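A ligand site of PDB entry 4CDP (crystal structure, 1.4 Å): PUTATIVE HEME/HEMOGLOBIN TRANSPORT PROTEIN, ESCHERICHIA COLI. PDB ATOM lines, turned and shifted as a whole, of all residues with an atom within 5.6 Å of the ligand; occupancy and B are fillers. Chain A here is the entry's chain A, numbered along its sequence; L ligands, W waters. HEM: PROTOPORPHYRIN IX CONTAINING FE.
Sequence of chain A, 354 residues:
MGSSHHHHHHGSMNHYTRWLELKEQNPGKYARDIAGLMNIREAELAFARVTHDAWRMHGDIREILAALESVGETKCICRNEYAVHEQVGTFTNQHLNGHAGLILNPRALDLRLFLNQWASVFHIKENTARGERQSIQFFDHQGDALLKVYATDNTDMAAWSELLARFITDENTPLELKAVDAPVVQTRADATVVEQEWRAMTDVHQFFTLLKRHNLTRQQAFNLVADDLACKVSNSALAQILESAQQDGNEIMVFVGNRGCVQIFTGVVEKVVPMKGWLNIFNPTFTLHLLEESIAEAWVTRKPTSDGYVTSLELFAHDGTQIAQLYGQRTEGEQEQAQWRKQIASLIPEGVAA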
ATOM      1  N   ALA A 100       3.177 -20.888  20.083  1.00  0.00           N
ATOM      2  CA  ALA A 100       4.502 -21.494  20.099  1.00  0.00           C
ATOM      3  C   ALA A 100       4.760 -21.862  21.548  1.00  0.00           C
ATOM      4  O   ALA A 100       4.053 -21.373  22.443  1.00  0.00           O
ATOM      5  CB  ALA A 100       5.535 -20.503  19.633  1.00  0.00           C
ATOM      6  N   GLY A 101       5.682 -22.804  21.757  1.00  0.00           N
ATOM      7  CA  GLY A 101       5.887 -23.300  23.098  1.00  0.00           C
ATOM      8  C   GLY A 101       7.101 -22.615  23.713  1.00  0.00           C
ATOM      9  O   GLY A 101       7.986 -22.067  23.028  1.00  0.00           O
ATOM     10  N   LEU A 102       7.108 -22.581  25.038  1.00  0.00           N
ATOM     11  CA  LEU A 102       8.336 -22.143  25.678  1.00  0.00           C
ATOM     12  C   LEU A 102       8.659 -22.874  26.961  1.00  0.00           C
ATOM     13  O   LEU A 102       7.767 -23.437  27.649  1.00  0.00           O
ATOM     14  CB  LEU A 102       8.488 -20.632  25.774  1.00  0.00           C
ATOM     15  CG  LEU A 102       7.666 -19.859  26.780  1.00  0.00           C
ATOM     16  CD1 LEU A 102       8.355 -18.495  26.873  1.00  0.00           C
ATOM     17  CD2 LEU A 102       6.264 -19.747  26.183  1.00  0.00           C
ATOM     18  N   LEU A 104      10.696 -21.676  30.069  1.00  0.00           N
ATOM     19  CA  LEU A 104      11.120 -20.323  30.417  1.00  0.00           C
ATOM     20  C   LEU A 104      12.000 -20.294  31.675  1.00  0.00           C
ATOM     21  O   LEU A 104      11.502 -20.351  32.805  1.00  0.00           O
ATOM     22  CB  LEU A 104       9.882 -19.442  30.639  1.00  0.00           C
ATOM     23  CG  LEU A 104      10.181 -17.967  30.980  1.00  0.00           C
ATOM     24  CD1 LEU A 104      10.967 -17.288  29.867  1.00  0.00           C
ATOM     25  CD2 LEU A 104       8.868 -17.216  31.221  1.00  0.00           C
ATOM     26  N   ARG A 112      12.562 -21.876  23.018  1.00  0.00           N
ATOM     27  CA  ARG A 112      11.339 -21.441  22.318  1.00  0.00           C
ATOM     28  C   ARG A 112      11.101 -22.523  21.261  1.00  0.00           C
ATOM     29  O   ARG A 112      12.029 -22.933  20.554  1.00  0.00           O
ATOM     30  CB  ARG A 112      11.516 -20.066  21.662  1.00  0.00           C
ATOM     31  CG  ARG A 112      12.000 -18.985  22.641  1.00  0.00           C
ATOM     32  CD  ARG A 112      11.016 -18.716  23.790  1.00  0.00           C
ATOM     33  NE  ARG A 112      11.561 -17.729  24.766  1.00  0.00           N
ATOM     34  CZ  ARG A 112      12.101 -18.030  25.952  1.00  0.00           C
ATOM     35  NH1 ARG A 112      12.135 -19.260  26.406  1.00  0.00           N
ATOM     36  NH2 ARG A 112      12.660 -17.099  26.690  1.00  0.00           N
ATOM     37  N   LEU A 113       9.883 -23.035  21.219  1.00  0.00           N
ATOM     38  CA  LEU A 113       9.589 -24.269  20.489  1.00  0.00           C
ATOM     39  C   LEU A 113       8.490 -24.053  19.449  1.00  0.00           C
ATOM     40  O   LEU A 113       7.422 -23.477  19.738  1.00  0.00           O
ATOM     41  CB  LEU A 113       9.191 -25.364  21.465  1.00  0.00           C
ATOM     42  CG  LEU A 113      10.034 -25.449  22.748  1.00  0.00           C
ATOM     43  CD1 LEU A 113       9.306 -26.296  23.774  1.00  0.00           C
ATOM     44  CD2 LEU A 113      11.386 -26.055  22.450  1.00  0.00           C
ATOM     45  N   PHE A 114       8.757 -24.517  18.222  1.00  0.00           N
ATOM     46  CA  PHE A 114       7.739 -24.476  17.178  1.00  0.00           C
ATOM     47  C   PHE A 114       7.288 -25.916  16.912  1.00  0.00           C
ATOM     48  O   PHE A 114       7.850 -26.605  16.043  1.00  0.00           O
ATOM     49  CB  PHE A 114       8.266 -23.761  15.940  1.00  0.00           C
ATOM     50  CG  PHE A 114       8.880 -22.412  16.259  1.00  0.00           C
ATOM     51  CD1 PHE A 114       8.117 -21.391  16.751  1.00  0.00           C
ATOM     52  CD2 PHE A 114      10.251 -22.254  16.188  1.00  0.00           C
ATOM     53  CE1 PHE A 114       8.691 -20.167  17.034  1.00  0.00           C
ATOM     54  CE2 PHE A 114      10.852 -21.045  16.552  1.00  0.00           C
ATOM     55  CZ  PHE A 114      10.064 -20.034  17.032  1.00  0.00           C
ATOM     56  N   VAL A 204       8.883  -6.787  19.975  1.00  0.00           N
ATOM     57  CA  VAL A 204       9.681  -7.524  18.964  1.00  0.00           C
ATOM     58  C   VAL A 204       9.023  -8.810  18.510  1.00  0.00           C
ATOM     59  O   VAL A 204       9.328  -9.317  17.413  1.00  0.00           O
ATOM     60  CB  VAL A 204      11.101  -7.855  19.454  1.00  0.00           C
ATOM     61  CG1 VAL A 204      11.826  -6.580  19.848  1.00  0.00           C
ATOM     62  CG2 VAL A 204      11.066  -8.877  20.594  1.00  0.00           C
ATOM     63  N   HIS A 205       8.118  -9.351  19.334  1.00  0.00           N
ATOM     64  CA  HIS A 205       7.483 -10.622  18.971  1.00  0.00           C
ATOM     65  C   HIS A 205       6.443 -10.484  17.843  1.00  0.00           C
ATOM     66  O   HIS A 205       5.909 -11.490  17.364  1.00  0.00           O
ATOM     67  CB  HIS A 205       6.883 -11.334  20.187  1.00  0.00           C
ATOM     68  CG  HIS A 205       7.878 -11.660  21.242  1.00  0.00           C
ATOM     69  ND1 HIS A 205       8.225 -10.774  22.252  1.00  0.00           N
ATOM     70  CD2 HIS A 205       8.690 -12.748  21.408  1.00  0.00           C
ATOM     71  CE1 HIS A 205       9.183 -11.303  23.000  1.00  0.00           C
ATOM     72  NE2 HIS A 205       9.488 -12.500  22.509  1.00  0.00           N
ATOM     73  N   PHE A 207       7.400  -9.072  15.007  1.00  0.00           N
ATOM     74  CA  PHE A 207       8.195  -8.919  13.784  1.00  0.00           C
ATOM     75  C   PHE A 207       8.052 -10.117  12.849  1.00  0.00           C
ATOM     76  O   PHE A 207       7.950  -9.948  11.634  1.00  0.00           O
ATOM     77  CB  PHE A 207       9.685  -8.690  14.133  1.00  0.00           C
ATOM     78  CG  PHE A 207      10.521  -8.364  12.931  1.00  0.00           C
ATOM     79  CD1 PHE A 207      10.220  -7.270  12.131  1.00  0.00           C
ATOM     80  CD2 PHE A 207      11.625  -9.170  12.581  1.00  0.00           C
ATOM     81  CE1 PHE A 207      10.995  -6.960  11.025  1.00  0.00           C
ATOM     82  CE2 PHE A 207      12.441  -8.838  11.519  1.00  0.00           C
ATOM     83  CZ  PHE A 207      12.127  -7.739  10.717  1.00  0.00           C
ATOM     84  N   ARG A 218      14.103 -12.350   6.558  1.00  0.00           N
ATOM     85  CA  ARG A 218      14.657 -11.285   7.399  1.00  0.00           C
ATOM     86  C   ARG A 218      15.519 -10.365   6.553  1.00  0.00           C
ATOM     87  O   ARG A 218      15.403  -9.152   6.644  1.00  0.00           O
ATOM     88  CB  ARG A 218      15.502 -11.863   8.560  1.00  0.00           C
ATOM     89  CG  ARG A 218      14.660 -12.765   9.474  1.00  0.00           C
ATOM     90  CD  ARG A 218      15.427 -13.163  10.730  1.00  0.00           C
ATOM     91  NE  ARG A 218      15.510 -12.092  11.700  1.00  0.00           N
ATOM     92  CZ  ARG A 218      14.556 -11.800  12.589  1.00  0.00           C
ATOM     93  NH1 ARG A 218      13.351 -12.353  12.503  1.00  0.00           N
ATOM     94  NH2 ARG A 218      14.768 -10.829  13.464  1.00  0.00           N
ATOM     95  N   MET A 253      22.233 -11.639  25.613  1.00  0.00           N
ATOM     96  CA  MET A 253      21.471 -12.818  25.219  1.00  0.00           C
ATOM     97  C   MET A 253      22.082 -13.339  23.926  1.00  0.00           C
ATOM     98  O   MET A 253      22.359 -12.561  22.998  1.00  0.00           O
ATOM     99  CB  MET A 253      20.027 -12.437  24.917  1.00  0.00           C
ATOM    100  CG  MET A 253      19.292 -11.759  26.093  1.00  0.00           C
ATOM    101  SD  MET A 253      17.631 -11.215  25.592  1.00  0.00           S
ATOM    102  CE  MET A 253      16.720 -12.750  25.644  1.00  0.00           C
ATOM    103  N   PHE A 255      21.036 -16.066  21.016  1.00  0.00           N
ATOM    104  CA  PHE A 255      19.969 -16.957  20.485  1.00  0.00           C
ATOM    105  C   PHE A 255      20.592 -17.794  19.381  1.00  0.00           C
ATOM    106  O   PHE A 255      21.199 -17.249  18.440  1.00  0.00           O
ATOM    107  CB  PHE A 255      18.866 -16.142  19.760  1.00  0.00           C
ATOM    108  CG  PHE A 255      18.014 -15.248  20.655  1.00  0.00           C
ATOM    109  CD1 PHE A 255      18.555 -14.152  21.370  1.00  0.00           C
ATOM    110  CD2 PHE A 255      16.628 -15.445  20.662  1.00  0.00           C
ATOM    111  CE1 PHE A 255      17.741 -13.293  22.087  1.00  0.00           C
ATOM    112  CE2 PHE A 255      15.795 -14.581  21.364  1.00  0.00           C
ATOM    113  CZ  PHE A 255      16.362 -13.517  22.075  1.00  0.00           C
ATOM    114  N   ILE A 264      18.298 -20.074  24.152  1.00  0.00           N
ATOM    115  CA  ILE A 264      18.692 -18.694  24.467  1.00  0.00           C
ATOM    116  C   ILE A 264      19.550 -18.663  25.719  1.00  0.00           C
ATOM    117  O   ILE A 264      19.122 -19.091  26.782  1.00  0.00           O
ATOM    118  CB  ILE A 264      17.447 -17.801  24.669  1.00  0.00           C
ATOM    119  CG1 ILE A 264      16.574 -17.808  23.377  1.00  0.00           C
ATOM    120  CG2 ILE A 264      17.861 -16.370  24.998  1.00  0.00           C
ATOM    121  CD1 ILE A 264      15.141 -17.382  23.595  1.00  0.00           C
ATOM    122  N   THR A 301      20.016  -4.291  14.002  1.00  0.00           N
ATOM    123  CA  THR A 301      18.618  -3.942  13.803  1.00  0.00           C
ATOM    124  C   THR A 301      18.026  -3.323  15.049  1.00  0.00           C
ATOM    125  O   THR A 301      18.397  -3.694  16.177  1.00  0.00           O
ATOM    126  CB  THR A 301      17.799  -5.190  13.389  1.00  0.00           C
ATOM    127  OG1 THR A 301      17.838  -6.181  14.442  1.00  0.00           O
ATOM    128  CG2 THR A 301      18.332  -5.796  12.107  1.00  0.00           C
ATOM    129  N   LYS A 303      14.280  -2.505  16.867  1.00  0.00           N
ATOM    130  CA  LYS A 303      12.848  -2.833  16.856  1.00  0.00           C
ATOM    131  C   LYS A 303      12.191  -2.271  18.115  1.00  0.00           C
ATOM    132  O   LYS A 303      12.790  -2.261  19.188  1.00  0.00           O
ATOM    133  CB  LYS A 303      12.644  -4.344  16.799  1.00  0.00           C
ATOM    134  CG  LYS A 303      13.275  -4.971  15.574  1.00  0.00           C
ATOM    135  CD  LYS A 303      12.925  -6.454  15.480  1.00  0.00           C
ATOM    136  CE  LYS A 303      13.879  -7.186  14.532  1.00  0.00           C
ATOM    137  NZ  LYS A 303      15.104  -7.633  15.240  1.00  0.00           N
ATOM    138  N   THR A 305       9.918  -1.784  21.474  1.00  0.00           N
ATOM    139  CA  THR A 305       9.254  -2.491  22.572  1.00  0.00           C
ATOM    140  C   THR A 305       8.180  -1.562  23.108  1.00  0.00           C
ATOM    141  O   THR A 305       8.047  -0.436  22.652  1.00  0.00           O
ATOM    142  CB  THR A 305      10.226  -2.801  23.714  1.00  0.00           C
ATOM    143  OG1 THR A 305      10.527  -1.593  24.426  1.00  0.00           O
ATOM    144  CG2 THR A 305      11.536  -3.399  23.173  1.00  0.00           C
ATOM    145  N   VAL A 310      14.797  -1.808  21.139  1.00  0.00           N
ATOM    146  CA  VAL A 310      15.968  -2.669  21.424  1.00  0.00           C
ATOM    147  C   VAL A 310      16.762  -2.902  20.150  1.00  0.00           C
ATOM    148  O   VAL A 310      16.252  -2.814  19.030  1.00  0.00           O
ATOM    149  CB  VAL A 310      15.552  -4.007  22.061  1.00  0.00           C
ATOM    150  CG1 VAL A 310      15.187  -3.801  23.541  1.00  0.00           C
ATOM    151  CG2 VAL A 310      14.400  -4.685  21.281  1.00  0.00           C
ATOM    152  N   SER A 312      19.612  -5.368  18.092  1.00  0.00           N
ATOM    153  CA  SER A 312      20.118  -6.730  17.938  1.00  0.00           C
ATOM    154  C   SER A 312      21.254  -6.787  16.938  1.00  0.00           C
ATOM    155  O   SER A 312      21.322  -6.002  15.978  1.00  0.00           O
ATOM    156  CB  SER A 312      18.973  -7.644  17.441  1.00  0.00           C
ATOM    157  OG  SER A 312      19.377  -9.012  17.463  1.00  0.00           O
ATOM    158  N   GLU A 314      22.415  -9.484  14.178  1.00  0.00           N
ATOM    159  CA  GLU A 314      21.829 -10.673  13.537  1.00  0.00           C
ATOM    160  C   GLU A 314      22.805 -11.180  12.478  1.00  0.00           C
ATOM    161  O   GLU A 314      23.264 -10.406  11.617  1.00  0.00           O
ATOM    162  CB  GLU A 314      20.488 -10.286  12.904  1.00  0.00           C
ATOM    163  CG  GLU A 314      19.531  -9.682  13.916  1.00  0.00           C
ATOM    164  CD  GLU A 314      18.071  -9.795  13.508  1.00  0.00           C
ATOM    165  OE1 GLU A 314      17.686 -10.814  12.893  1.00  0.00           O
ATOM    166  OE2 GLU A 314      17.294  -8.850  13.790  1.00  0.00           O
ATOM    167  N   GLN A 325      21.660 -14.713  16.874  1.00  0.00           N
ATOM    168  CA  GLN A 325      21.239 -13.339  17.114  1.00  0.00           C
ATOM    169  C   GLN A 325      21.618 -12.987  18.530  1.00  0.00           C
ATOM    170  O   GLN A 325      21.503 -13.815  19.426  1.00  0.00           O
ATOM    171  CB  GLN A 325      19.699 -13.277  16.933  1.00  0.00           C
ATOM    172  CG  GLN A 325      19.025 -12.028  17.347  1.00  0.00           C
ATOM    173  CD  GLN A 325      17.590 -11.965  16.911  1.00  0.00           C
ATOM    174  OE1 GLN A 325      16.890 -12.996  16.713  1.00  0.00           O
ATOM    175  NE2 GLN A 325      17.148 -10.749  16.721  1.00  0.00           N
ATOM    176  N   TYR A 327      21.305  -9.904  21.734  1.00  0.00           N
ATOM    177  CA  TYR A 327      20.682  -8.729  22.349  1.00  0.00           C
ATOM    178  C   TYR A 327      21.406  -8.481  23.659  1.00  0.00           C
ATOM    179  O   TYR A 327      22.183  -9.300  24.133  1.00  0.00           O
ATOM    180  CB  TYR A 327      19.211  -9.021  22.672  1.00  0.00           C
ATOM    181  CG  TYR A 327      18.224  -8.736  21.559  1.00  0.00           C
ATOM    182  CD1 TYR A 327      17.816  -7.425  21.315  1.00  0.00           C
ATOM    183  CD2 TYR A 327      17.597  -9.760  20.843  1.00  0.00           C
ATOM    184  CE1 TYR A 327      16.860  -7.135  20.359  1.00  0.00           C
ATOM    185  CE2 TYR A 327      16.582  -9.470  19.913  1.00  0.00           C
ATOM    186  CZ  TYR A 327      16.273  -8.146  19.671  1.00  0.00           C
ATOM    187  OH  TYR A 327      15.274  -7.843  18.773  1.00  0.00           O
ATOM    188  N   GLY A 328      21.130  -7.317  24.270  1.00  0.00           N
ATOM    189  CA  GLY A 328      21.462  -7.145  25.683  1.00  0.00           C
ATOM    190  C   GLY A 328      20.432  -7.854  26.540  1.00  0.00           C
ATOM    191  O   GLY A 328      19.286  -8.059  26.110  1.00  0.00           O
ATOM    192  N   ARG A 330      17.478  -7.909  29.073  1.00  0.00           N
ATOM    193  CA  ARG A 330      16.446  -6.879  29.382  1.00  0.00           C
ATOM    194  C   ARG A 330      15.219  -7.521  30.001  1.00  0.00           C
ATOM    195  O   ARG A 330      14.789  -8.571  29.538  1.00  0.00           O
ATOM    196  CB  ARG A 330      16.014  -6.110  28.101  1.00  0.00           C
ATOM    197  CG  ARG A 330      15.245  -4.822  28.432  1.00  0.00           C
ATOM    198  CD  ARG A 330      14.703  -4.184  27.146  1.00  0.00           C
ATOM    199  NE  ARG A 330      13.641  -4.954  26.527  1.00  0.00           N
ATOM    200  CZ  ARG A 330      12.340  -4.800  26.788  1.00  0.00           C
ATOM    201  NH1 ARG A 330      11.959  -3.963  27.747  1.00  0.00           N
ATOM    202  NH2 ARG A 330      11.458  -5.599  26.183  1.00  0.00           N
HETATM  203  CHA HEM L   1      13.164 -11.692  21.679  1.00  0.00           C
HETATM  204  CHB HEM L   1      11.495 -12.292  26.237  1.00  0.00           C
HETATM  205  CHC HEM L   1       8.292 -15.555  24.485  1.00  0.00           C
HETATM  206  CHD HEM L   1      10.931 -15.843  20.416  1.00  0.00           C
HETATM  207  C1A HEM L   1      12.985 -11.580  23.062  1.00  0.00           C
HETATM  208  C2A HEM L   1      13.659 -10.636  23.897  1.00  0.00           C
HETATM  209  C3A HEM L   1      13.234 -10.825  25.181  1.00  0.00           C
HETATM  210  C4A HEM L   1      12.218 -11.848  25.130  1.00  0.00           C
HETATM  211  CMA HEM L   1      13.711 -10.095  26.420  1.00  0.00           C
HETATM  212  CAA HEM L   1      14.744  -9.658  23.454  1.00  0.00           C
HETATM  213  CBA HEM L   1      14.137  -8.333  22.896  1.00  0.00           C
HETATM  214  CGA HEM L   1      13.588  -7.463  24.013  1.00  0.00           C
HETATM  215  O1A HEM L   1      12.362  -7.185  24.010  1.00  0.00           O
HETATM  216  O2A HEM L   1      14.338  -7.018  24.925  1.00  0.00           O
HETATM  217  C1B HEM L   1      10.407 -13.193  26.140  1.00  0.00           C
HETATM  218  C2B HEM L   1       9.514 -13.519  27.213  1.00  0.00           C
HETATM  219  C3B HEM L   1       8.620 -14.441  26.737  1.00  0.00           C
HETATM  220  C4B HEM L   1       8.994 -14.689  25.323  1.00  0.00           C
HETATM  221  CMB HEM L   1       9.529 -12.946  28.625  1.00  0.00           C
HETATM  222  CAB HEM L   1       7.447 -15.045  27.409  1.00  0.00           C
HETATM  223  CBB HEM L   1       7.223 -14.821  28.696  1.00  0.00           C
HETATM  224  C1C HEM L   1       8.716 -15.958  23.219  1.00  0.00           C
HETATM  225  C2C HEM L   1       8.150 -16.994  22.430  1.00  0.00           C
HETATM  226  C3C HEM L   1       8.919 -17.040  21.282  1.00  0.00           C
HETATM  227  C4C HEM L   1       9.977 -16.098  21.384  1.00  0.00           C
HETATM  228  CMC HEM L   1       6.941 -17.864  22.772  1.00  0.00           C
HETATM  229  CAC HEM L   1       8.760 -17.933  20.097  1.00  0.00           C
HETATM  230  CBC HEM L   1       8.486 -19.244  20.223  1.00  0.00           C
HETATM  231  C1D HEM L   1      11.734 -14.684  20.460  1.00  0.00           C
HETATM  232  C2D HEM L   1      12.488 -14.253  19.269  1.00  0.00           C
HETATM  233  C3D HEM L   1      13.068 -13.084  19.612  1.00  0.00           C
HETATM  234  C4D HEM L   1      12.674 -12.817  21.004  1.00  0.00           C
HETATM  235  CMD HEM L   1      12.603 -14.997  17.948  1.00  0.00           C
HETATM  236  CAD HEM L   1      13.895 -12.171  18.719  1.00  0.00           C
HETATM  237  CBD HEM L   1      12.911 -11.257  17.957  1.00  0.00           C
HETATM  238  CGD HEM L   1      13.565 -10.451  16.848  1.00  0.00           C
HETATM  239  O1D HEM L   1      13.123 -10.568  15.675  1.00  0.00           O
HETATM  240  O2D HEM L   1      14.487  -9.627  17.041  1.00  0.00           O
HETATM  241  NA  HEM L   1      12.084 -12.319  23.816  1.00  0.00           N
HETATM  242  NB  HEM L   1      10.041 -13.899  25.045  1.00  0.00           N
HETATM  243  NC  HEM L   1       9.838 -15.441  22.578  1.00  0.00           N
HETATM  244  ND  HEM L   1      11.871 -13.799  21.469  1.00  0.00           N
HETATM  245 FE   HEM L   1      10.974 -13.832  23.191  1.00  0.00          FE
HETATM  246  O   HOH W   1       9.884  -6.515  22.793  1.00  0.00           O
HETATM  247  O   HOH W   2      13.056 -10.874  29.738  1.00  0.00           O
HETATM  248  O   HOH W   3      17.018  -7.003  24.722  1.00  0.00           O
HETATM  249  O   HOH W   4      11.477 -12.385  14.824  1.00  0.00           O
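A ring nitrogen (NE2) of His 205 binds an iron atom (FE) of the ligand (2.1 Å). OH of Tyr 327 is in hydrogen-bond range of O2D of the ligand (2.6 Å). NE of Arg 330 is in salt-bridge range of O2A of the ligand. An oxygen (O2D) of the ligand lies within salt-bridge range of the side-chain amino group of Lys 303, 2.8 Å away. NH2 of Arg 218 lies within salt-bridge range of O1D of the ligand (2.8 Å). An oxygen (O2D) of the ligand lies within hydrogen-bond range of the side-chain amide nitrogen of Gln 325 (2.9 Å).
The backbone NH of Met 253 sits at hydrogen-bond distance from the backbone carbonyl oxygen of Tyr 327 (2.8 Å). The backbone carbonyl oxygen (O) of Lys 303 sits at hydrogen-bond distance from the backbone NH (N) of Val 310 (2.8 Å). NZ of Lys 303 lies within salt-bridge range of OE2 of Glu 314. The side-chain hydroxyl of Thr 301 sits at hydrogen-bond distance from the side-chain amino group of Lys 303 (3.2 Å). NE of Arg 218 lies within salt-bridge range of OE1 of Glu 314. The backbone carbonyl oxygen (O) of Gln 325 is in hydrogen-bond range of the backbone NH (N) of Phe 255, 2.8 Å away. NE2 of Gln 325 lies close to OE2 of Glu 314 (3.5 Å). NE2 of Gln 325 sits at hydrogen-bond distance from OG of Ser 312 (2.9 Å).
Merely in contact with the ligand: Ala 100, Leu 102, Leu 104, Arg 112, Phe 114, Val 204, Phe 207, Met 253, Phe 255, Thr 305 and Val 310. Hydrophobic or aromatic side chains within 4 Å of the ligand: Ala 100, Leu 102, Leu 104, Phe 114, Val 204, His 205, Phe 207, Met 253, Phe 255, Val 310 and Tyr 327. Of the 24 residues printed, 17 come within 4 Å of the ligand.
Water W4 lies within hydrogen-bond range of an oxygen (O1D) of the ligand (2.6 Å) and the guanidinium group (NH1) of Arg 218 (3.0 Å). Water W3 lies within hydrogen-bond range of an oxygen (O2A) of the ligand (2.7 Å) and the backbone carbonyl oxygen of Gly 328 (2.9 Å). Water W1 lies within hydrogen-bond range of O1A of the ligand and N of Val 204.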
